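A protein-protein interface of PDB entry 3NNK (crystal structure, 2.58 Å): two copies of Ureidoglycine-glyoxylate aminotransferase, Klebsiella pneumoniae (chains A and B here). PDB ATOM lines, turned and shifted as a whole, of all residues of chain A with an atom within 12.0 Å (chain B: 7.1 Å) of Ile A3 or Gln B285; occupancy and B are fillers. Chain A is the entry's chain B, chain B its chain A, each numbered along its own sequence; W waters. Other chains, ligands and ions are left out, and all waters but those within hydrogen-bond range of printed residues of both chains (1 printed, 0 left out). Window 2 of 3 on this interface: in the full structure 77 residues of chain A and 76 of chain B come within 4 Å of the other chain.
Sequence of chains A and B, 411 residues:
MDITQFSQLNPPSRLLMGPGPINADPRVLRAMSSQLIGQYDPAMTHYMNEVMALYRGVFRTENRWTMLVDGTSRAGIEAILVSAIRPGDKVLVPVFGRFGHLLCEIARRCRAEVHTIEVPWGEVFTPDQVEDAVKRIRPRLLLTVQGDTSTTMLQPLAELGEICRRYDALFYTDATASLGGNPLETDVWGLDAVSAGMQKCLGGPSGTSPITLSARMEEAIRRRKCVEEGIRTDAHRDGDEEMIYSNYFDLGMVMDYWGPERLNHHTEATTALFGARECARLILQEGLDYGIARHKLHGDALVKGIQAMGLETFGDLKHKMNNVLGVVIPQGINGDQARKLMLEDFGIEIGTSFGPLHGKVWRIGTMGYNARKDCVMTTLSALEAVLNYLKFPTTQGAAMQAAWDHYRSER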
ATOM      1  N   ASP A   2       6.053  -3.052 -12.669  1.00  0.00           N
ATOM      2  CA  ASP A   2       5.312  -1.759 -12.744  1.00  0.00           C
ATOM      3  C   ASP A   2       4.258  -1.666 -11.646  1.00  0.00           C
ATOM      4  O   ASP A   2       3.595  -2.653 -11.325  1.00  0.00           O
ATOM      5  CB  ASP A   2       4.660  -1.590 -14.118  1.00  0.00           C
ATOM      6  N   ILE A   3       4.109  -0.472 -11.077  1.00  0.00           N
ATOM      7  CA  ILE A   3       3.169  -0.230  -9.974  1.00  0.00           C
ATOM      8  C   ILE A   3       1.733   0.052 -10.454  1.00  0.00           C
ATOM      9  O   ILE A   3       0.798   0.103  -9.648  1.00  0.00           O
ATOM     10  CB  ILE A   3       3.679   0.901  -9.020  1.00  0.00           C
ATOM     11  CG1 ILE A   3       2.673   1.195  -7.904  1.00  0.00           C
ATOM     12  CG2 ILE A   3       3.992   2.180  -9.788  1.00  0.00           C
ATOM     13  CD1 ILE A   3       3.051   0.532  -6.567  1.00  0.00           C
ATOM     14  N   THR A   4       1.562   0.212 -11.765  1.00  0.00           N
ATOM     15  CA  THR A   4       0.243   0.454 -12.356  1.00  0.00           C
ATOM     16  C   THR A   4      -0.669  -0.777 -12.316  1.00  0.00           C
ATOM     17  O   THR A   4      -1.894  -0.640 -12.265  1.00  0.00           O
ATOM     18  CB  THR A   4       0.346   0.978 -13.805  1.00  0.00           C
ATOM     19  OG1 THR A   4       1.437   0.333 -14.477  1.00  0.00           O
ATOM     20  CG2 THR A   4       0.579   2.482 -13.812  1.00  0.00           C
ATOM     21  N   GLN A   5      -0.071  -1.968 -12.334  1.00  0.00           N
ATOM     22  CA  GLN A   5      -0.832  -3.222 -12.240  1.00  0.00           C
ATOM     23  C   GLN A   5      -1.077  -3.664 -10.789  1.00  0.00           C
ATOM     24  O   GLN A   5      -1.451  -4.812 -10.529  1.00  0.00           O
ATOM     25  CB  GLN A   5      -0.176  -4.336 -13.068  1.00  0.00           C
ATOM     26  CG  GLN A   5       1.289  -4.609 -12.751  1.00  0.00           C
ATOM     27  CD  GLN A   5       2.038  -5.212 -13.927  1.00  0.00           C
ATOM     28  OE1 GLN A   5       2.782  -6.182 -13.772  1.00  0.00           O
ATOM     29  NE2 GLN A   5       1.846  -4.640 -15.113  1.00  0.00           N
ATOM     30  N   PHE A   6      -0.853  -2.740  -9.858  1.00  0.00           N
ATOM     31  CA  PHE A   6      -1.241  -2.911  -8.465  1.00  0.00           C
ATOM     32  C   PHE A   6      -2.393  -1.953  -8.183  1.00  0.00           C
ATOM     33  O   PHE A   6      -2.184  -0.814  -7.755  1.00  0.00           O
ATOM     34  CB  PHE A   6      -0.057  -2.638  -7.531  1.00  0.00           C
ATOM     35  CG  PHE A   6       0.963  -3.743  -7.499  1.00  0.00           C
ATOM     36  CD1 PHE A   6       2.014  -3.768  -8.413  1.00  0.00           C
ATOM     37  CD2 PHE A   6       0.878  -4.756  -6.549  1.00  0.00           C
ATOM     38  CE1 PHE A   6       2.963  -4.790  -8.384  1.00  0.00           C
ATOM     39  CE2 PHE A   6       1.823  -5.782  -6.511  1.00  0.00           C
ATOM     40  CZ  PHE A   6       2.868  -5.798  -7.430  1.00  0.00           C
ATOM     41  N   SER A   7      -3.610  -2.421  -8.449  1.00  0.00           N
ATOM     42  CA  SER A   7      -4.803  -1.580  -8.371  1.00  0.00           C
ATOM     43  C   SER A   7      -5.394  -1.532  -6.963  1.00  0.00           C
ATOM     44  O   SER A   7      -4.912  -2.217  -6.056  1.00  0.00           O
ATOM     45  CB  SER A   7      -5.853  -2.053  -9.380  1.00  0.00           C
ATOM     46  OG  SER A   7      -6.086  -3.444  -9.256  1.00  0.00           O
ATOM     47  N   GLN A   8      -6.436  -0.717  -6.797  1.00  0.00           N
ATOM     48  CA  GLN A   8      -7.111  -0.548  -5.510  1.00  0.00           C
ATOM     49  C   GLN A   8      -7.639  -1.870  -4.956  1.00  0.00           C
ATOM     50  O   GLN A   8      -7.868  -2.825  -5.708  1.00  0.00           O
ATOM     51  CB  GLN A   8      -8.241   0.482  -5.617  1.00  0.00           C
ATOM     52  CG  GLN A   8      -9.444   0.048  -6.454  1.00  0.00           C
ATOM     53  CD  GLN A   8     -10.631   0.983  -6.305  1.00  0.00           C
ATOM     54  OE1 GLN A   8     -10.834   1.590  -5.252  1.00  0.00           O
ATOM     55  NE2 GLN A   8     -11.431   1.094  -7.361  1.00  0.00           N
ATOM     56  N   LEU A   9      -7.821  -1.913  -3.638  1.00  0.00           N
ATOM     57  CA  LEU A   9      -8.294  -3.109  -2.952  1.00  0.00           C
ATOM     58  C   LEU A   9      -9.688  -3.491  -3.442  1.00  0.00           C
ATOM     59  O   LEU A   9     -10.618  -2.682  -3.400  1.00  0.00           O
ATOM     60  CB  LEU A   9      -8.292  -2.893  -1.432  1.00  0.00           C
ATOM     61  CG  LEU A   9      -7.888  -4.030  -0.480  1.00  0.00           C
ATOM     62  CD1 LEU A   9      -8.987  -5.063  -0.302  1.00  0.00           C
ATOM     63  CD2 LEU A   9      -6.579  -4.703  -0.898  1.00  0.00           C
ATOM     64  N   ARG B  27      -6.916   7.055   1.958  1.00  0.00           N
ATOM     65  CA  ARG B  27      -7.038   5.881   1.081  1.00  0.00           C
ATOM     66  C   ARG B  27      -6.738   4.574   1.822  1.00  0.00           C
ATOM     67  O   ARG B  27      -7.334   3.535   1.530  1.00  0.00           O
ATOM     68  CB  ARG B  27      -6.143   6.003  -0.158  1.00  0.00           C
ATOM     69  CG  ARG B  27      -6.496   7.168  -1.081  1.00  0.00           C
ATOM     70  CD  ARG B  27      -5.372   8.180  -1.146  1.00  0.00           C
ATOM     71  NE  ARG B  27      -4.595   8.076  -2.380  1.00  0.00           N
ATOM     72  CZ  ARG B  27      -3.398   8.629  -2.572  1.00  0.00           C
ATOM     73  NH1 ARG B  27      -2.806   9.322  -1.605  1.00  0.00           N
ATOM     74  NH2 ARG B  27      -2.783   8.477  -3.737  1.00  0.00           N
ATOM     75  N   LEU B  54       5.723  -5.649  -3.238  1.00  0.00           N
ATOM     76  CA  LEU B  54       5.576  -4.222  -2.951  1.00  0.00           C
ATOM     77  C   LEU B  54       6.548  -3.739  -1.879  1.00  0.00           C
ATOM     78  O   LEU B  54       7.130  -2.661  -2.011  1.00  0.00           O
ATOM     79  CB  LEU B  54       4.136  -3.877  -2.549  1.00  0.00           C
ATOM     80  CG  LEU B  54       3.087  -3.712  -3.654  1.00  0.00           C
ATOM     81  CD1 LEU B  54       1.688  -3.692  -3.060  1.00  0.00           C
ATOM     82  CD2 LEU B  54       3.337  -2.465  -4.484  1.00  0.00           C
ATOM     83  N   GLU B 278      -1.795  -0.904   1.016  1.00  0.00           N
ATOM     84  CA  GLU B 278      -1.997   0.450   0.489  1.00  0.00           C
ATOM     85  C   GLU B 278      -0.799   1.351   0.737  1.00  0.00           C
ATOM     86  O   GLU B 278      -0.288   1.969  -0.194  1.00  0.00           O
ATOM     87  CB  GLU B 278      -3.253   1.099   1.078  1.00  0.00           C
ATOM     88  CG  GLU B 278      -4.517   0.861   0.283  1.00  0.00           C
ATOM     89  CD  GLU B 278      -4.389   1.257  -1.178  1.00  0.00           C
ATOM     90  OE1 GLU B 278      -4.164   2.453  -1.466  1.00  0.00           O
ATOM     91  OE2 GLU B 278      -4.529   0.363  -2.038  1.00  0.00           O
ATOM     92  N   CYS B 279      -0.355   1.416   1.992  1.00  0.00           N
ATOM     93  CA  CYS B 279       0.784   2.246   2.380  1.00  0.00           C
ATOM     94  C   CYS B 279       1.944   2.119   1.392  1.00  0.00           C
ATOM     95  O   CYS B 279       2.403   3.120   0.838  1.00  0.00           O
ATOM     96  CB  CYS B 279       1.248   1.895   3.793  1.00  0.00           C
ATOM     97  SG  CYS B 279       0.051   2.287   5.077  1.00  0.00           S
ATOM     98  N   ALA B 280       2.385   0.884   1.162  1.00  0.00           N
ATOM     99  CA  ALA B 280       3.471   0.586   0.230  1.00  0.00           C
ATOM    100  C   ALA B 280       3.103   0.914  -1.215  1.00  0.00           C
ATOM    101  O   ALA B 280       3.938   1.410  -1.973  1.00  0.00           O
ATOM    102  CB  ALA B 280       3.881  -0.871   0.350  1.00  0.00           C
ATOM    103  N   ARG B 281       1.856   0.633  -1.588  1.00  0.00           N
ATOM    104  CA  ARG B 281       1.364   0.893  -2.940  1.00  0.00           C
ATOM    105  C   ARG B 281       1.391   2.388  -3.254  1.00  0.00           C
ATOM    106  O   ARG B 281       1.879   2.794  -4.309  1.00  0.00           O
ATOM    107  CB  ARG B 281      -0.049   0.334  -3.107  1.00  0.00           C
ATOM    108  CG  ARG B 281      -0.473   0.090  -4.546  1.00  0.00           C
ATOM    109  CD  ARG B 281      -1.867  -0.524  -4.601  1.00  0.00           C
ATOM    110  NE  ARG B 281      -2.895   0.402  -4.128  1.00  0.00           N
ATOM    111  CZ  ARG B 281      -3.644   1.169  -4.916  1.00  0.00           C
ATOM    112  NH1 ARG B 281      -3.504   1.125  -6.233  1.00  0.00           N
ATOM    113  NH2 ARG B 281      -4.546   1.982  -4.381  1.00  0.00           N
ATOM    114  N   LEU B 282       0.879   3.194  -2.325  1.00  0.00           N
ATOM    115  CA  LEU B 282       0.857   4.649  -2.469  1.00  0.00           C
ATOM    116  C   LEU B 282       2.266   5.235  -2.498  1.00  0.00           C
ATOM    117  O   LEU B 282       2.559   6.105  -3.321  1.00  0.00           O
ATOM    118  CB  LEU B 282       0.036   5.301  -1.348  1.00  0.00           C
ATOM    119  CG  LEU B 282      -1.420   4.870  -1.127  1.00  0.00           C
ATOM    120  CD1 LEU B 282      -1.959   5.480   0.158  1.00  0.00           C
ATOM    121  CD2 LEU B 282      -2.319   5.221  -2.313  1.00  0.00           C
ATOM    122  N   ILE B 283       3.133   4.750  -1.607  1.00  0.00           N
ATOM    123  CA  ILE B 283       4.527   5.200  -1.546  1.00  0.00           C
ATOM    124  C   ILE B 283       5.247   5.000  -2.883  1.00  0.00           C
ATOM    125  O   ILE B 283       6.030   5.856  -3.307  1.00  0.00           O
ATOM    126  CB  ILE B 283       5.312   4.521  -0.385  1.00  0.00           C
ATOM    127  CG1 ILE B 283       4.935   5.160   0.958  1.00  0.00           C
ATOM    128  CG2 ILE B 283       6.831   4.622  -0.606  1.00  0.00           C
ATOM    129  CD1 ILE B 283       5.336   4.343   2.175  1.00  0.00           C
ATOM    130  N   LEU B 284       4.957   3.887  -3.554  1.00  0.00           N
ATOM    131  CA  LEU B 284       5.605   3.564  -4.828  1.00  0.00           C
ATOM    132  C   LEU B 284       4.927   4.187  -6.058  1.00  0.00           C
ATOM    133  O   LEU B 284       5.494   4.164  -7.154  1.00  0.00           O
ATOM    134  CB  LEU B 284       5.751   2.047  -4.994  1.00  0.00           C
ATOM    135  CG  LEU B 284       6.646   1.293  -4.005  1.00  0.00           C
ATOM    136  CD1 LEU B 284       6.409  -0.202  -4.128  1.00  0.00           C
ATOM    137  CD2 LEU B 284       8.126   1.626  -4.203  1.00  0.00           C
ATOM    138  N   GLN B 285       3.724   4.734  -5.878  1.00  0.00           N
ATOM    139  CA  GLN B 285       3.052   5.486  -6.940  1.00  0.00           C
ATOM    140  C   GLN B 285       3.675   6.875  -7.066  1.00  0.00           C
ATOM    141  O   GLN B 285       3.964   7.341  -8.172  1.00  0.00           O
ATOM    142  CB  GLN B 285       1.547   5.596  -6.677  1.00  0.00           C
ATOM    143  CG  GLN B 285       0.756   4.324  -6.978  1.00  0.00           C
ATOM    144  CD  GLN B 285      -0.752   4.525  -6.896  1.00  0.00           C
ATOM    145  OE1 GLN B 285      -1.240   5.650  -6.770  1.00  0.00           O
ATOM    146  NE2 GLN B 285      -1.496   3.428  -6.978  1.00  0.00           N
ATOM    147  N   GLU B 286       3.875   7.521  -5.919  1.00  0.00           N
ATOM    148  CA  GLU B 286       4.589   8.793  -5.828  1.00  0.00           C
ATOM    149  C   GLU B 286       6.076   8.585  -6.113  1.00  0.00           C
ATOM    150  O   GLU B 286       6.723   9.425  -6.742  1.00  0.00           O
ATOM    151  CB  GLU B 286       4.397   9.399  -4.432  1.00  0.00           C
ATOM    152  CG  GLU B 286       5.166  10.695  -4.161  1.00  0.00           C
ATOM    153  CD  GLU B 286       5.270  11.029  -2.677  1.00  0.00           C
ATOM    154  OE1 GLU B 286       4.910  10.177  -1.833  1.00  0.00           O
ATOM    155  OE2 GLU B 286       5.716  12.150  -2.352  1.00  0.00           O
ATOM    156  N   GLY B 287       6.602   7.453  -5.652  1.00  0.00           N
ATOM    157  CA  GLY B 287       8.021   7.133  -5.785  1.00  0.00           C
ATOM    158  C   GLY B 287       8.756   7.408  -4.487  1.00  0.00           C
ATOM    159  O   GLY B 287       8.646   8.501  -3.924  1.00  0.00           O
ATOM    160  N   LEU B 288       9.501   6.413  -4.012  1.00  0.00           N
ATOM    161  CA  LEU B 288      10.244   6.523  -2.755  1.00  0.00           C
ATOM    162  C   LEU B 288      11.195   7.723  -2.747  1.00  0.00           C
ATOM    163  O   LEU B 288      11.235   8.480  -1.775  1.00  0.00           O
ATOM    164  CB  LEU B 288      10.998   5.220  -2.455  1.00  0.00           C
ATOM    165  CG  LEU B 288      11.825   5.121  -1.168  1.00  0.00           C
ATOM    166  CD1 LEU B 288      10.947   5.053   0.079  1.00  0.00           C
ATOM    167  CD2 LEU B 288      12.766   3.928  -1.228  1.00  0.00           C
ATOM    168  N   TYR B 290      10.922  10.495  -4.284  1.00  0.00           N
ATOM    169  CA  TYR B 290      10.136  11.720  -4.118  1.00  0.00           C
ATOM    170  C   TYR B 290       9.475  11.804  -2.746  1.00  0.00           C
ATOM    171  O   TYR B 290       9.252  12.900  -2.226  1.00  0.00           O
ATOM    172  CB  TYR B 290       9.089  11.859  -5.224  1.00  0.00           C
ATOM    173  CG  TYR B 290       9.676  12.143  -6.589  1.00  0.00           C
ATOM    174  CD1 TYR B 290      10.590  13.182  -6.776  1.00  0.00           C
ATOM    175  CD2 TYR B 290       9.306  11.382  -7.698  1.00  0.00           C
ATOM    176  CE1 TYR B 290      11.132  13.451  -8.028  1.00  0.00           C
ATOM    177  CE2 TYR B 290       9.841  11.644  -8.958  1.00  0.00           C
ATOM    178  CZ  TYR B 290      10.754  12.681  -9.115  1.00  0.00           C
ATOM    179  OH  TYR B 290      11.289  12.953 -10.354  1.00  0.00           O
HETATM  180  O   HOH W   1      -7.150   0.045  -1.924  1.00  0.00           O
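NH1 of Arg B281 sits at hydrogen-bond distance from O of Phe A6 (2.8 Å).
Of chain A, only Ile A3 comes within 4 Å of Gln B285. No residue of chain A comes within 4 Å of Ala B280. Arg B281 touches just these residues of chain A: Ile A3, Phe A6, Ser A7 and Gln A8. No residue of chain A comes within 4 Å of Leu B282. Printed residues of chain A within 4 Å of Leu B284: Ile A3. No residue of chain A comes within 4 Å of Glu B286. No residue of chain A comes within 4 Å of Gly B287. Of the printed residues of chain B, Ser A7 touches Arg B281 (3.3 Å). Printed residues of chain B within 4 Å of Gln A8: Arg B281. Of the printed residues of chain B, Phe A6 touches Leu B54 and Arg B281. The nearest residue of chain A that does not touch Gln B285 is Phe A6 (4.4 Å).
NH1 of Arg B281 sits close to NE2 of Gln B285, at 3.1 Å. OE2 of Glu B278 lies within salt-bridge range of NE of Arg B281 (2.7 Å).
Of the 14 printed residues of chain B, 4 touch a printed residue of chain A. Printed residues of chain B that touch a printed residue of chain A: Leu B54, Arg B281, Leu B284 and Gln B285. Of the 8 printed residues of chain A, 4 touch a printed residue of chain B. Among the printed residues, no Asp or Glu carboxylate lies within 4 Å of a Lys or Arg side-chain nitrogen of the other chain.
Water W1 lies within hydrogen-bond range of the side-chain carboxylate of Glu B278 and the backbone NH of Leu A9.
Among the printed residues, merely in contact across the chains: Ser A7 with Arg B281, Ile A3 with Arg B281, Ile A3 with Leu B284, Gln A8 with Arg B281, Ile A3 with Leu B54, Phe A6 with Leu B54 and Ile A3 with Gln B285.
No position is printed for both chains.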
